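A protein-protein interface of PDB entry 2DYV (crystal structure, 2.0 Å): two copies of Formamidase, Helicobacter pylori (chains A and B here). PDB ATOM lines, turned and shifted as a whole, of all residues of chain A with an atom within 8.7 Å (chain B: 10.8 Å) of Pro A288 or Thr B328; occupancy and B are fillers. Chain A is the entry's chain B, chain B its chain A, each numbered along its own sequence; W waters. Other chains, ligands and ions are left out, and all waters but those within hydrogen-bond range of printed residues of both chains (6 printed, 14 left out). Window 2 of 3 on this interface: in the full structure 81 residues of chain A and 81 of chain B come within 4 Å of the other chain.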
ATOM      1  N   TYR A 277     -19.519 -12.634 -19.591  1.00  0.00           N
ATOM      2  CA  TYR A 277     -20.930 -12.377 -19.908  1.00  0.00           C
ATOM      3  C   TYR A 277     -21.649 -13.628 -20.387  1.00  0.00           C
ATOM      4  O   TYR A 277     -22.804 -13.885 -20.007  1.00  0.00           O
ATOM      5  CB  TYR A 277     -21.059 -11.276 -20.965  1.00  0.00           C
ATOM      6  CG  TYR A 277     -22.494 -10.913 -21.275  1.00  0.00           C
ATOM      7  CD1 TYR A 277     -23.211 -10.062 -20.439  1.00  0.00           C
ATOM      8  CD2 TYR A 277     -23.134 -11.430 -22.399  1.00  0.00           C
ATOM      9  CE1 TYR A 277     -24.529  -9.720 -20.723  1.00  0.00           C
ATOM     10  CE2 TYR A 277     -24.445 -11.106 -22.689  1.00  0.00           C
ATOM     11  CZ  TYR A 277     -25.137 -10.247 -21.846  1.00  0.00           C
ATOM     12  OH  TYR A 277     -26.432  -9.940 -22.142  1.00  0.00           O
ATOM     13  N   HIS A 281     -25.417 -15.848 -19.848  1.00  0.00           N
ATOM     14  CA  HIS A 281     -26.227 -15.467 -20.992  1.00  0.00           C
ATOM     15  C   HIS A 281     -25.953 -16.330 -22.220  1.00  0.00           C
ATOM     16  O   HIS A 281     -25.771 -15.796 -23.313  1.00  0.00           O
ATOM     17  CB  HIS A 281     -26.026 -13.977 -21.309  1.00  0.00           C
ATOM     18  CG  HIS A 281     -26.471 -13.065 -20.206  1.00  0.00           C
ATOM     19  ND1 HIS A 281     -25.611 -12.586 -19.242  1.00  0.00           N
ATOM     20  CD2 HIS A 281     -27.696 -12.587 -19.887  1.00  0.00           C
ATOM     21  CE1 HIS A 281     -26.281 -11.820 -18.397  1.00  0.00           C
ATOM     22  NE2 HIS A 281     -27.553 -11.811 -18.764  1.00  0.00           N
ATOM     23  N   ARG A 282     -25.981 -17.654 -22.038  1.00  0.00           N
ATOM     24  CA  ARG A 282     -25.564 -18.620 -23.066  1.00  0.00           C
ATOM     25  C   ARG A 282     -26.442 -18.489 -24.312  1.00  0.00           C
ATOM     26  O   ARG A 282     -27.662 -18.532 -24.221  1.00  0.00           O
ATOM     27  CB  ARG A 282     -25.719 -20.069 -22.573  1.00  0.00           C
ATOM     28  CG  ARG A 282     -25.403 -20.337 -21.117  1.00  0.00           C
ATOM     29  CD  ARG A 282     -26.138 -21.584 -20.618  1.00  0.00           C
ATOM     30  NE  ARG A 282     -26.250 -22.490 -21.723  1.00  0.00           N
ATOM     31  CZ  ARG A 282     -27.167 -23.425 -21.888  1.00  0.00           C
ATOM     32  NH1 ARG A 282     -28.113 -23.676 -20.997  1.00  0.00           N
ATOM     33  NH2 ARG A 282     -27.100 -24.117 -22.989  1.00  0.00           N
ATOM     34  N   GLY A 283     -25.813 -18.352 -25.470  1.00  0.00           N
ATOM     35  CA  GLY A 283     -26.534 -18.390 -26.734  1.00  0.00           C
ATOM     36  C   GLY A 283     -27.486 -17.238 -27.004  1.00  0.00           C
ATOM     37  O   GLY A 283     -28.546 -17.453 -27.585  1.00  0.00           O
ATOM     38  N   TYR A 284     -27.107 -16.018 -26.631  1.00  0.00           N
ATOM     39  CA  TYR A 284     -28.003 -14.853 -26.746  1.00  0.00           C
ATOM     40  C   TYR A 284     -28.394 -14.444 -28.188  1.00  0.00           C
ATOM     41  O   TYR A 284     -29.317 -13.650 -28.367  1.00  0.00           O
ATOM     42  CB  TYR A 284     -27.461 -13.635 -25.958  1.00  0.00           C
ATOM     43  CG  TYR A 284     -26.127 -13.106 -26.454  1.00  0.00           C
ATOM     44  CD1 TYR A 284     -26.025 -12.425 -27.670  1.00  0.00           C
ATOM     45  CD2 TYR A 284     -24.968 -13.287 -25.706  1.00  0.00           C
ATOM     46  CE1 TYR A 284     -24.796 -11.952 -28.132  1.00  0.00           C
ATOM     47  CE2 TYR A 284     -23.740 -12.822 -26.161  1.00  0.00           C
ATOM     48  CZ  TYR A 284     -23.662 -12.147 -27.367  1.00  0.00           C
ATOM     49  OH  TYR A 284     -22.441 -11.697 -27.816  1.00  0.00           O
ATOM     50  N   VAL A 285     -27.707 -14.974 -29.204  1.00  0.00           N
ATOM     51  CA  VAL A 285     -28.064 -14.665 -30.595  1.00  0.00           C
ATOM     52  C   VAL A 285     -29.362 -15.386 -30.961  1.00  0.00           C
ATOM     53  O   VAL A 285     -30.276 -14.784 -31.512  1.00  0.00           O
ATOM     54  CB  VAL A 285     -26.929 -15.029 -31.595  1.00  0.00           C
ATOM     55  CG1 VAL A 285     -27.420 -14.967 -33.041  1.00  0.00           C
ATOM     56  CG2 VAL A 285     -25.730 -14.120 -31.389  1.00  0.00           C
ATOM     57  N   ALA A 286     -29.434 -16.674 -30.619  1.00  0.00           N
ATOM     58  CA  ALA A 286     -30.600 -17.494 -30.875  1.00  0.00           C
ATOM     59  C   ALA A 286     -31.728 -17.240 -29.875  1.00  0.00           C
ATOM     60  O   ALA A 286     -32.910 -17.365 -30.217  1.00  0.00           O
ATOM     61  CB  ALA A 286     -30.212 -18.976 -30.851  1.00  0.00           C
ATOM     62  N   LYS A 287     -31.369 -16.907 -28.638  1.00  0.00           N
ATOM     63  CA  LYS A 287     -32.361 -16.739 -27.575  1.00  0.00           C
ATOM     64  C   LYS A 287     -32.118 -15.417 -26.875  1.00  0.00           C
ATOM     65  O   LYS A 287     -31.141 -15.284 -26.142  1.00  0.00           O
ATOM     66  CB  LYS A 287     -32.289 -17.907 -26.578  1.00  0.00           C
ATOM     67  CG  LYS A 287     -33.271 -17.858 -25.429  1.00  0.00           C
ATOM     68  CD  LYS A 287     -33.010 -19.016 -24.468  1.00  0.00           C
ATOM     69  CE  LYS A 287     -34.242 -19.321 -23.636  1.00  0.00           C
ATOM     70  NZ  LYS A 287     -34.603 -18.200 -22.747  1.00  0.00           N
ATOM     71  N   PRO A 288     -33.009 -14.428 -27.099  1.00  0.00           N
ATOM     72  CA  PRO A 288     -32.854 -13.088 -26.531  1.00  0.00           C
ATOM     73  C   PRO A 288     -32.534 -13.155 -25.035  1.00  0.00           C
ATOM     74  O   PRO A 288     -33.235 -13.825 -24.281  1.00  0.00           O
ATOM     75  CB  PRO A 288     -34.223 -12.456 -26.782  1.00  0.00           C
ATOM     76  CG  PRO A 288     -34.653 -13.090 -28.090  1.00  0.00           C
ATOM     77  CD  PRO A 288     -34.221 -14.526 -27.941  1.00  0.00           C
ATOM     78  N   GLY A 289     -31.446 -12.506 -24.634  1.00  0.00           N
ATOM     79  CA  GLY A 289     -31.023 -12.471 -23.243  1.00  0.00           C
ATOM     80  C   GLY A 289     -30.093 -13.606 -22.867  1.00  0.00           C
ATOM     81  O   GLY A 289     -29.408 -13.537 -21.844  1.00  0.00           O
ATOM     82  N   GLY A 290     -30.080 -14.646 -23.701  1.00  0.00           N
ATOM     83  CA  GLY A 290     -29.341 -15.867 -23.435  1.00  0.00           C
ATOM     84  C   GLY A 290     -30.141 -16.777 -22.522  1.00  0.00           C
ATOM     85  O   GLY A 290     -31.157 -16.367 -21.936  1.00  0.00           O
ATOM     86  N   GLU A 291     -29.693 -18.022 -22.417  1.00  0.00           N
ATOM     87  CA  GLU A 291     -30.233 -18.960 -21.443  1.00  0.00           C
ATOM     88  C   GLU A 291     -29.552 -18.683 -20.090  1.00  0.00           C
ATOM     89  O   GLU A 291     -28.324 -18.684 -19.985  1.00  0.00           O
ATOM     90  CB  GLU A 291     -30.056 -20.408 -21.957  1.00  0.00           C
ATOM     91  CG  GLU A 291     -30.439 -21.531 -21.009  1.00  0.00           C
ATOM     92  CD  GLU A 291     -31.859 -21.439 -20.485  1.00  0.00           C
ATOM     93  OE1 GLU A 291     -32.812 -21.722 -21.234  1.00  0.00           O
ATOM     94  OE2 GLU A 291     -32.021 -21.113 -19.304  1.00  0.00           O
ATOM     95  N   HIS A 292     -30.363 -18.386 -19.077  1.00  0.00           N
ATOM     96  CA  HIS A 292     -29.868 -17.945 -17.763  1.00  0.00           C
ATOM     97  C   HIS A 292     -29.484 -19.108 -16.848  1.00  0.00           C
ATOM     98  O   HIS A 292     -28.791 -18.919 -15.846  1.00  0.00           O
ATOM     99  CB  HIS A 292     -30.901 -17.032 -17.081  1.00  0.00           C
ATOM    100  CG  HIS A 292     -31.087 -15.722 -17.782  1.00  0.00           C
ATOM    101  ND1 HIS A 292     -32.003 -15.543 -18.795  1.00  0.00           N
ATOM    102  CD2 HIS A 292     -30.448 -14.538 -17.639  1.00  0.00           C
ATOM    103  CE1 HIS A 292     -31.937 -14.298 -19.230  1.00  0.00           C
ATOM    104  NE2 HIS A 292     -30.992 -13.670 -18.554  1.00  0.00           N
ATOM    105  N   ASN B 111     -39.723 -23.642 -33.745  1.00  0.00           N
ATOM    106  CA  ASN B 111     -39.649 -22.240 -33.364  1.00  0.00           C
ATOM    107  C   ASN B 111     -38.293 -21.857 -32.811  1.00  0.00           C
ATOM    108  O   ASN B 111     -38.122 -20.746 -32.302  1.00  0.00           O
ATOM    109  CB  ASN B 111     -40.732 -21.917 -32.332  1.00  0.00           C
ATOM    110  CG  ASN B 111     -42.121 -22.080 -32.894  1.00  0.00           C
ATOM    111  OD1 ASN B 111     -42.438 -21.539 -33.950  1.00  0.00           O
ATOM    112  ND2 ASN B 111     -42.962 -22.837 -32.195  1.00  0.00           N
ATOM    113  N   LYS B 112     -37.335 -22.778 -32.919  1.00  0.00           N
ATOM    114  CA  LYS B 112     -36.007 -22.594 -32.344  1.00  0.00           C
ATOM    115  C   LYS B 112     -34.937 -22.934 -33.379  1.00  0.00           C
ATOM    116  O   LYS B 112     -35.124 -23.811 -34.224  1.00  0.00           O
ATOM    117  CB  LYS B 112     -35.818 -23.489 -31.114  1.00  0.00           C
ATOM    118  CG  LYS B 112     -36.541 -23.082 -29.826  1.00  0.00           C
ATOM    119  CD  LYS B 112     -36.154 -24.079 -28.712  1.00  0.00           C
ATOM    120  CE  LYS B 112     -36.801 -23.749 -27.371  1.00  0.00           C
ATOM    121  NZ  LYS B 112     -36.334 -24.690 -26.309  1.00  0.00           N
ATOM    122  N   ASN B 113     -33.810 -22.238 -33.303  1.00  0.00           N
ATOM    123  CA  ASN B 113     -32.683 -22.504 -34.194  1.00  0.00           C
ATOM    124  C   ASN B 113     -32.059 -23.886 -33.949  1.00  0.00           C
ATOM    125  O   ASN B 113     -32.229 -24.464 -32.865  1.00  0.00           O
ATOM    126  CB  ASN B 113     -31.634 -21.397 -34.052  1.00  0.00           C
ATOM    127  CG  ASN B 113     -31.923 -20.196 -34.933  1.00  0.00           C
ATOM    128  OD1 ASN B 113     -32.927 -20.151 -35.655  1.00  0.00           O
ATOM    129  ND2 ASN B 113     -31.038 -19.216 -34.888  1.00  0.00           N
ATOM    130  N   ASN B 138     -20.835 -16.289 -29.472  1.00  0.00           N
ATOM    131  CA  ASN B 138     -21.636 -15.125 -29.804  1.00  0.00           C
ATOM    132  C   ASN B 138     -20.776 -13.862 -29.898  1.00  0.00           C
ATOM    133  O   ASN B 138     -19.814 -13.716 -29.136  1.00  0.00           O
ATOM    134  CB  ASN B 138     -22.728 -14.918 -28.753  1.00  0.00           C
ATOM    135  CG  ASN B 138     -23.750 -16.042 -28.713  1.00  0.00           C
ATOM    136  OD1 ASN B 138     -24.135 -16.625 -29.736  1.00  0.00           O
ATOM    137  ND2 ASN B 138     -24.200 -16.352 -27.520  1.00  0.00           N
ATOM    138  N   GLU B 141     -22.219 -16.899 -33.898  1.00  0.00           N
ATOM    139  CA  GLU B 141     -22.973 -18.165 -34.061  1.00  0.00           C
ATOM    140  C   GLU B 141     -24.453 -18.072 -33.686  1.00  0.00           C
ATOM    141  O   GLU B 141     -24.804 -17.537 -32.634  1.00  0.00           O
ATOM    142  CB  GLU B 141     -22.319 -19.326 -33.286  1.00  0.00           C
ATOM    143  CG  GLU B 141     -20.978 -19.768 -33.848  1.00  0.00           C
ATOM    144  CD  GLU B 141     -20.321 -20.916 -33.074  1.00  0.00           C
ATOM    145  OE1 GLU B 141     -20.809 -21.328 -31.999  1.00  0.00           O
ATOM    146  OE2 GLU B 141     -19.288 -21.409 -33.556  1.00  0.00           O
ATOM    147  N   PRO B 142     -25.329 -18.620 -34.547  1.00  0.00           N
ATOM    148  CA  PRO B 142     -26.773 -18.578 -34.341  1.00  0.00           C
ATOM    149  C   PRO B 142     -27.360 -19.832 -33.666  1.00  0.00           C
ATOM    150  O   PRO B 142     -28.597 -19.971 -33.593  1.00  0.00           O
ATOM    151  CB  PRO B 142     -27.287 -18.508 -35.779  1.00  0.00           C
ATOM    152  CG  PRO B 142     -26.340 -19.436 -36.522  1.00  0.00           C
ATOM    153  CD  PRO B 142     -24.986 -19.285 -35.820  1.00  0.00           C
ATOM    154  N   TRP B 143     -26.502 -20.738 -33.204  1.00  0.00           N
ATOM    155  CA  TRP B 143     -26.966 -22.009 -32.635  1.00  0.00           C
ATOM    156  C   TRP B 143     -27.737 -21.773 -31.345  1.00  0.00           C
ATOM    157  O   TRP B 143     -27.361 -20.918 -30.541  1.00  0.00           O
ATOM    158  CB  TRP B 143     -25.790 -22.975 -32.393  1.00  0.00           C
ATOM    159  CG  TRP B 143     -24.842 -23.030 -33.571  1.00  0.00           C
ATOM    160  CD1 TRP B 143     -23.527 -22.633 -33.599  1.00  0.00           C
ATOM    161  CD2 TRP B 143     -25.153 -23.485 -34.895  1.00  0.00           C
ATOM    162  NE1 TRP B 143     -23.003 -22.819 -34.864  1.00  0.00           N
ATOM    163  CE2 TRP B 143     -23.980 -23.341 -35.675  1.00  0.00           C
ATOM    164  CE3 TRP B 143     -26.306 -24.020 -35.494  1.00  0.00           C
ATOM    165  CZ2 TRP B 143     -23.931 -23.704 -37.022  1.00  0.00           C
ATOM    166  CZ3 TRP B 143     -26.254 -24.377 -36.844  1.00  0.00           C
ATOM    167  CH2 TRP B 143     -25.074 -24.212 -37.591  1.00  0.00           C
ATOM    168  N   TYR B 144     -28.819 -22.532 -31.169  1.00  0.00           N
ATOM    169  CA  TYR B 144     -29.581 -22.516 -29.923  1.00  0.00           C
ATOM    170  C   TYR B 144     -28.713 -23.046 -28.772  1.00  0.00           C
ATOM    171  O   TYR B 144     -28.028 -24.050 -28.949  1.00  0.00           O
ATOM    172  CB  TYR B 144     -30.892 -23.322 -30.055  1.00  0.00           C
ATOM    173  CG  TYR B 144     -31.977 -22.716 -29.191  1.00  0.00           C
ATOM    174  CD1 TYR B 144     -32.739 -21.645 -29.660  1.00  0.00           C
ATOM    175  CD2 TYR B 144     -32.175 -23.148 -27.877  1.00  0.00           C
ATOM    176  CE1 TYR B 144     -33.693 -21.038 -28.856  1.00  0.00           C
ATOM    177  CE2 TYR B 144     -33.116 -22.549 -27.063  1.00  0.00           C
ATOM    178  CZ  TYR B 144     -33.875 -21.493 -27.561  1.00  0.00           C
ATOM    179  OH  TYR B 144     -34.827 -20.899 -26.776  1.00  0.00           O
ATOM    180  N   PRO B 145     -28.728 -22.366 -27.595  1.00  0.00           N
ATOM    181  CA  PRO B 145     -27.932 -22.848 -26.470  1.00  0.00           C
ATOM    182  C   PRO B 145     -28.382 -24.246 -26.057  1.00  0.00           C
ATOM    183  O   PRO B 145     -29.589 -24.515 -25.956  1.00  0.00           O
ATOM    184  CB  PRO B 145     -28.220 -21.817 -25.359  1.00  0.00           C
ATOM    185  CG  PRO B 145     -29.539 -21.180 -25.752  1.00  0.00           C
ATOM    186  CD  PRO B 145     -29.470 -21.134 -27.242  1.00  0.00           C
ATOM    187  N   GLU B 312     -23.458  -4.779 -17.107  1.00  0.00           N
ATOM    188  CA  GLU B 312     -24.325  -5.205 -18.214  1.00  0.00           C
ATOM    189  C   GLU B 312     -25.032  -4.028 -18.888  1.00  0.00           C
ATOM    190  O   GLU B 312     -25.178  -4.007 -20.117  1.00  0.00           O
ATOM    191  CB  GLU B 312     -25.337  -6.267 -17.757  1.00  0.00           C
ATOM    192  CG  GLU B 312     -24.671  -7.560 -17.356  1.00  0.00           C
ATOM    193  CD  GLU B 312     -25.602  -8.762 -17.281  1.00  0.00           C
ATOM    194  OE1 GLU B 312     -26.775  -8.689 -17.703  1.00  0.00           O
ATOM    195  OE2 GLU B 312     -25.125  -9.800 -16.803  1.00  0.00           O
ATOM    196  N   ILE B 317     -22.429  -5.289 -26.953  1.00  0.00           N
ATOM    197  CA  ILE B 317     -22.828  -6.479 -27.716  1.00  0.00           C
ATOM    198  C   ILE B 317     -23.603  -7.488 -26.856  1.00  0.00           C
ATOM    199  O   ILE B 317     -23.027  -8.235 -26.049  1.00  0.00           O
ATOM    200  CB  ILE B 317     -21.626  -7.143 -28.432  1.00  0.00           C
ATOM    201  CG1 ILE B 317     -20.925  -6.121 -29.342  1.00  0.00           C
ATOM    202  CG2 ILE B 317     -22.108  -8.368 -29.238  1.00  0.00           C
ATOM    203  CD1 ILE B 317     -19.655  -6.616 -30.018  1.00  0.00           C
ATOM    204  N   LYS B 318     -24.921  -7.484 -27.027  1.00  0.00           N
ATOM    205  CA  LYS B 318     -25.795  -8.335 -26.239  1.00  0.00           C
ATOM    206  C   LYS B 318     -26.805  -9.056 -27.124  1.00  0.00           C
ATOM    207  O   LYS B 318     -27.724  -9.713 -26.631  1.00  0.00           O
ATOM    208  CB  LYS B 318     -26.498  -7.514 -25.151  1.00  0.00           C
ATOM    209  CG  LYS B 318     -25.540  -6.939 -24.095  1.00  0.00           C
ATOM    210  CD  LYS B 318     -26.285  -6.409 -22.867  1.00  0.00           C
ATOM    211  CE  LYS B 318     -26.902  -5.048 -23.121  1.00  0.00           C
ATOM    212  NZ  LYS B 318     -27.480  -4.484 -21.857  1.00  0.00           N
ATOM    213  N   ASP B 319     -26.617  -8.920 -28.433  1.00  0.00           N
ATOM    214  CA  ASP B 319     -27.412  -9.629 -29.426  1.00  0.00           C
ATOM    215  C   ASP B 319     -26.580  -9.803 -30.701  1.00  0.00           C
ATOM    216  O   ASP B 319     -25.433  -9.361 -30.745  1.00  0.00           O
ATOM    217  CB  ASP B 319     -28.750  -8.909 -29.695  1.00  0.00           C
ATOM    218  CG  ASP B 319     -28.577  -7.473 -30.204  1.00  0.00           C
ATOM    219  OD1 ASP B 319     -27.693  -7.227 -31.051  1.00  0.00           O
ATOM    220  OD2 ASP B 319     -29.354  -6.591 -29.772  1.00  0.00           O
ATOM    221  N   GLY B 320     -27.150 -10.441 -31.725  1.00  0.00           N
ATOM    222  CA  GLY B 320     -26.439 -10.654 -32.986  1.00  0.00           C
ATOM    223  C   GLY B 320     -26.591  -9.569 -34.045  1.00  0.00           C
ATOM    224  O   GLY B 320     -26.294  -9.809 -35.230  1.00  0.00           O
ATOM    225  N   SER B 321     -27.031  -8.378 -33.635  1.00  0.00           N
ATOM    226  CA  SER B 321     -27.334  -7.308 -34.595  1.00  0.00           C
ATOM    227  C   SER B 321     -26.112  -6.882 -35.430  1.00  0.00           C
ATOM    228  O   SER B 321     -26.251  -6.585 -36.618  1.00  0.00           O
ATOM    229  CB  SER B 321     -28.021  -6.110 -33.920  1.00  0.00           C
ATOM    230  OG  SER B 321     -27.154  -5.443 -33.026  1.00  0.00           O
ATOM    231  N   GLY B 324     -26.069  -8.983 -38.368  1.00  0.00           N
ATOM    232  CA  GLY B 324     -27.260  -8.937 -39.212  1.00  0.00           C
ATOM    233  C   GLY B 324     -28.387  -9.840 -38.755  1.00  0.00           C
ATOM    234  O   GLY B 324     -29.439  -9.862 -39.369  1.00  0.00           O
ATOM    235  N   TYR B 325     -28.172 -10.571 -37.659  1.00  0.00           N
ATOM    236  CA  TYR B 325     -29.195 -11.464 -37.116  1.00  0.00           C
ATOM    237  C   TYR B 325     -30.367 -10.712 -36.489  1.00  0.00           C
ATOM    238  O   TYR B 325     -30.173  -9.650 -35.886  1.00  0.00           O
ATOM    239  CB  TYR B 325     -28.601 -12.394 -36.062  1.00  0.00           C
ATOM    240  CG  TYR B 325     -27.504 -13.293 -36.552  1.00  0.00           C
ATOM    241  CD1 TYR B 325     -27.699 -14.141 -37.644  1.00  0.00           C
ATOM    242  CD2 TYR B 325     -26.266 -13.316 -35.908  1.00  0.00           C
ATOM    243  CE1 TYR B 325     -26.679 -14.987 -38.081  1.00  0.00           C
ATOM    244  CE2 TYR B 325     -25.255 -14.151 -36.330  1.00  0.00           C
ATOM    245  CZ  TYR B 325     -25.463 -14.981 -37.417  1.00  0.00           C
ATOM    246  OH  TYR B 325     -24.442 -15.803 -37.841  1.00  0.00           O
ATOM    247  N   PRO B 326     -31.588 -11.262 -36.625  1.00  0.00           N
ATOM    248  CA  PRO B 326     -32.717 -10.645 -35.926  1.00  0.00           C
ATOM    249  C   PRO B 326     -32.542 -10.767 -34.422  1.00  0.00           C
ATOM    250  O   PRO B 326     -31.859 -11.678 -33.948  1.00  0.00           O
ATOM    251  CB  PRO B 326     -33.926 -11.450 -36.407  1.00  0.00           C
ATOM    252  CG  PRO B 326     -33.370 -12.735 -36.910  1.00  0.00           C
ATOM    253  CD  PRO B 326     -31.994 -12.429 -37.428  1.00  0.00           C
ATOM    254  N   THR B 327     -33.140  -9.843 -33.684  1.00  0.00           N
ATOM    255  CA  THR B 327     -32.907  -9.735 -32.247  1.00  0.00           C
ATOM    256  C   THR B 327     -34.107 -10.160 -31.402  1.00  0.00           C
ATOM    257  O   THR B 327     -34.075 -10.066 -30.177  1.00  0.00           O
ATOM    258  CB  THR B 327     -32.520  -8.289 -31.875  1.00  0.00           C
ATOM    259  OG1 THR B 327     -33.560  -7.398 -32.300  1.00  0.00           O
ATOM    260  CG2 THR B 327     -31.210  -7.894 -32.567  1.00  0.00           C
ATOM    261  N   THR B 328     -35.160 -10.641 -32.054  1.00  0.00           N
ATOM    262  CA  THR B 328     -36.442 -10.833 -31.366  1.00  0.00           C
ATOM    263  C   THR B 328     -36.777 -12.272 -31.033  1.00  0.00           C
ATOM    264  O   THR B 328     -37.798 -12.530 -30.392  1.00  0.00           O
ATOM    265  CB  THR B 328     -37.613 -10.205 -32.151  1.00  0.00           C
ATOM    266  OG1 THR B 328     -37.612 -10.699 -33.495  1.00  0.00           O
ATOM    267  CG2 THR B 328     -37.477  -8.699 -32.167  1.00  0.00           C
ATOM    268  N   GLY B 329     -35.930 -13.204 -31.460  1.00  0.00           N
ATOM    269  CA  GLY B 329     -36.128 -14.615 -31.157  1.00  0.00           C
ATOM    270  C   GLY B 329     -36.702 -15.422 -32.311  1.00  0.00           C
ATOM    271  O   GLY B 329     -36.856 -14.921 -33.429  1.00  0.00           O
ATOM    272  N   GLY B 330     -37.005 -16.685 -32.031  1.00  0.00           N
ATOM    273  CA  GLY B 330     -37.591 -17.573 -33.020  1.00  0.00           C
ATOM    274  C   GLY B 330     -36.580 -18.147 -33.990  1.00  0.00           C
ATOM    275  O   GLY B 330     -35.377 -17.872 -33.890  1.00  0.00           O
ATOM    276  N   ARG B 331     -37.086 -18.956 -34.918  1.00  0.00           N
ATOM    277  CA  ARG B 331     -36.280 -19.591 -35.953  1.00  0.00           C
ATOM    278  C   ARG B 331     -35.944 -18.589 -37.055  1.00  0.00           C
ATOM    279  O   ARG B 331     -36.823 -17.881 -37.552  1.00  0.00           O
ATOM    280  CB  ARG B 331     -37.047 -20.789 -36.526  1.00  0.00           C
ATOM    281  CG  ARG B 331     -36.391 -21.502 -37.711  1.00  0.00           C
ATOM    282  CD  ARG B 331     -35.113 -22.211 -37.308  1.00  0.00           C
ATOM    283  NE  ARG B 331     -34.774 -23.275 -38.250  1.00  0.00           N
ATOM    284  CZ  ARG B 331     -33.812 -23.205 -39.167  1.00  0.00           C
ATOM    285  NH1 ARG B 331     -33.054 -22.120 -39.276  1.00  0.00           N
ATOM    286  NH2 ARG B 331     -33.599 -24.235 -39.971  1.00  0.00           N
ATOM    287  N   PHE B 332     -34.668 -18.509 -37.427  1.00  0.00           N
ATOM    288  CA  PHE B 332     -34.270 -17.696 -38.576  1.00  0.00           C
ATOM    289  C   PHE B 332     -33.217 -18.372 -39.467  1.00  0.00           C
ATOM    290  O   PHE B 332     -32.720 -19.450 -39.143  1.00  0.00           O
ATOM    291  CB  PHE B 332     -33.860 -16.271 -38.151  1.00  0.00           C
ATOM    292  CG  PHE B 332     -32.694 -16.202 -37.183  1.00  0.00           C
ATOM    293  CD1 PHE B 332     -31.387 -16.290 -37.642  1.00  0.00           C
ATOM    294  CD2 PHE B 332     -32.911 -15.997 -35.822  1.00  0.00           C
ATOM    295  CE1 PHE B 332     -30.304 -16.205 -36.754  1.00  0.00           C
ATOM    296  CE2 PHE B 332     -31.839 -15.905 -34.933  1.00  0.00           C
ATOM    297  CZ  PHE B 332     -30.531 -16.010 -35.405  1.00  0.00           C
HETATM  298  O   HOH W   1     -27.871  -8.581 -20.244  1.00  0.00           O
HETATM  299  O   HOH W   2     -20.508 -12.132 -26.101  1.00  0.00           O
HETATM  300  O   HOH W   3     -33.741 -19.546 -32.211  1.00  0.00           O
HETATM  301  O   HOH W   4     -29.926 -11.262 -26.935  1.00  0.00           O
HETATM  302  O   HOH W   5     -33.004 -13.196 -31.843  1.00  0.00           O
HETATM  303  O   HOH W   6     -35.684 -17.496 -29.668  1.00  0.00           O
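A ring nitrogen (NE2) of His A281 sits close to the side-chain carboxylate (OE1) of Glu B312 (3.4 Å).
The backbone NH (N) of Tyr A284 sits close to the side-chain amide nitrogen (ND2) of Asn B138.
ND2 of Asn B138 sits close to N of Gly A283, at 3.3 Å.
The backbone carbonyl oxygen of Arg A282 lies within hydrogen-bond range of the backbone NH of Glu A291.
The side-chain amide oxygen (OD1) of Asn B138 lies close to the backbone carbonyl oxygen (O) of Glu B141 (3.1 Å).
O of Pro B142 sits at hydrogen-bond distance from ND2 of Asn B113.
OD1 of Asp B319 sits at hydrogen-bond distance from OG of Ser B321.
The backbone carbonyl oxygen (O) of Glu B312 lies within hydrogen-bond range of the side-chain amino group (NZ) of Lys B318 (2.9 Å).
N of Tyr B325 is in hydrogen-bond range of O of Gly B320 (3.2 Å).
C of Pro B145 touches NH2 of Arg A282, at 3.3 Å.
Gly A283 touches Pro B145 (O to CD, 3.8 Å).
Tyr A284 touches Lys B318.
Asp B319 touches Tyr A284 (N to CE1, 3.5 Å).
O of Glu B141 touches CB of Val A285, at 3.4 Å.
CA of Pro B142 touches CG1 of Val A285, at 3.9 Å.
O of Val A285 touches CE2 of Phe B332, 3.9 Å away.
Trp B143 touches Ala A286 (O to CB, 3.5 Å).
CA of Tyr B144 touches CB of Ala A286 (3.7 Å).
Gly B329 touches Pro A288.
Printed residues of chain B within 4 Å of His A281: Glu B312 (2.8 Å).
Lys A287 touches just one residue of chain B: Tyr B144.
Pro A288 touches just these residues of chain B: Thr B327, Thr B328 and Gly B329.
Gly A289 touches none of the printed residues of chain B.
No residue of chain B comes within 4 Å of Gly A290.
Of the printed residues of chain A, Pro B142 touches Val A285 (3.9 Å) and Ala A286 (3.3 Å).
Printed residues of chain A within 4 Å of Tyr B144: Ala A286 and Lys A287.
Thr B328 touches just one residue of chain A: Pro A288 (3.7 Å).
Gly B329 touches just one residue of chain A: Pro A288 (3.6 Å).
Hydrophobic or aromatic side chains of chain A within 4 Å of the printed part of chain B: Tyr A277, His A281, Tyr A284, Val A285, Ala A286 and Pro A288.
Of the 24 printed residues of chain B, 16 touch a printed residue of chain A.
Printed residues of chain B that touch a printed residue of chain A: Asn B138, Glu B141, Pro B142, Trp B143, Tyr B144, Pro B145, Glu B312, Ile B317, Lys B318, Asp B319, Gly B320, Tyr B325, Thr B327, Thr B328, Gly B329 and Phe B332.
Hydrophobic or aromatic side chains of chain B within 4 Å of the printed part of chain A: Tyr B144, Pro B145, Ile B317, Tyr B325 and Phe B332.
Among the printed residues, no Asp or Glu carboxylate lies within 4 Å of a Lys or Arg side-chain nitrogen of the other chain.
No position is printed for both chains.
Water W2 lies within hydrogen-bond range of the side-chain hydroxyl of Tyr A284 (2.6 Å) and the backbone carbonyl oxygen of Asn B138 (3.5 Å).
Water W4 lies within hydrogen-bond range of O of Lys B318, O of Tyr A284 and N of Gly A289.
Water W1 lies within hydrogen-bond range of OH of Tyr A277 (2.7 Å) and OE1 of Glu B312 (2.8 Å).
Water W6 lies within hydrogen-bond range of the backbone NH (N) of Gly B330 (2.8 Å) and the backbone carbonyl oxygen (O) of Ala A286 (2.8 Å).
Water W5 lies within hydrogen-bond range of O of Pro B326 (2.8 Å), N of Gly B329 (3.0 Å), O of Val A285 (3.2 Å) and N of Thr B328 (3.3 Å).
Water W3 lies within hydrogen-bond range of the backbone carbonyl oxygen of Gly B330, the backbone NH of Asn B113 and the backbone carbonyl oxygen of Ala A286.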
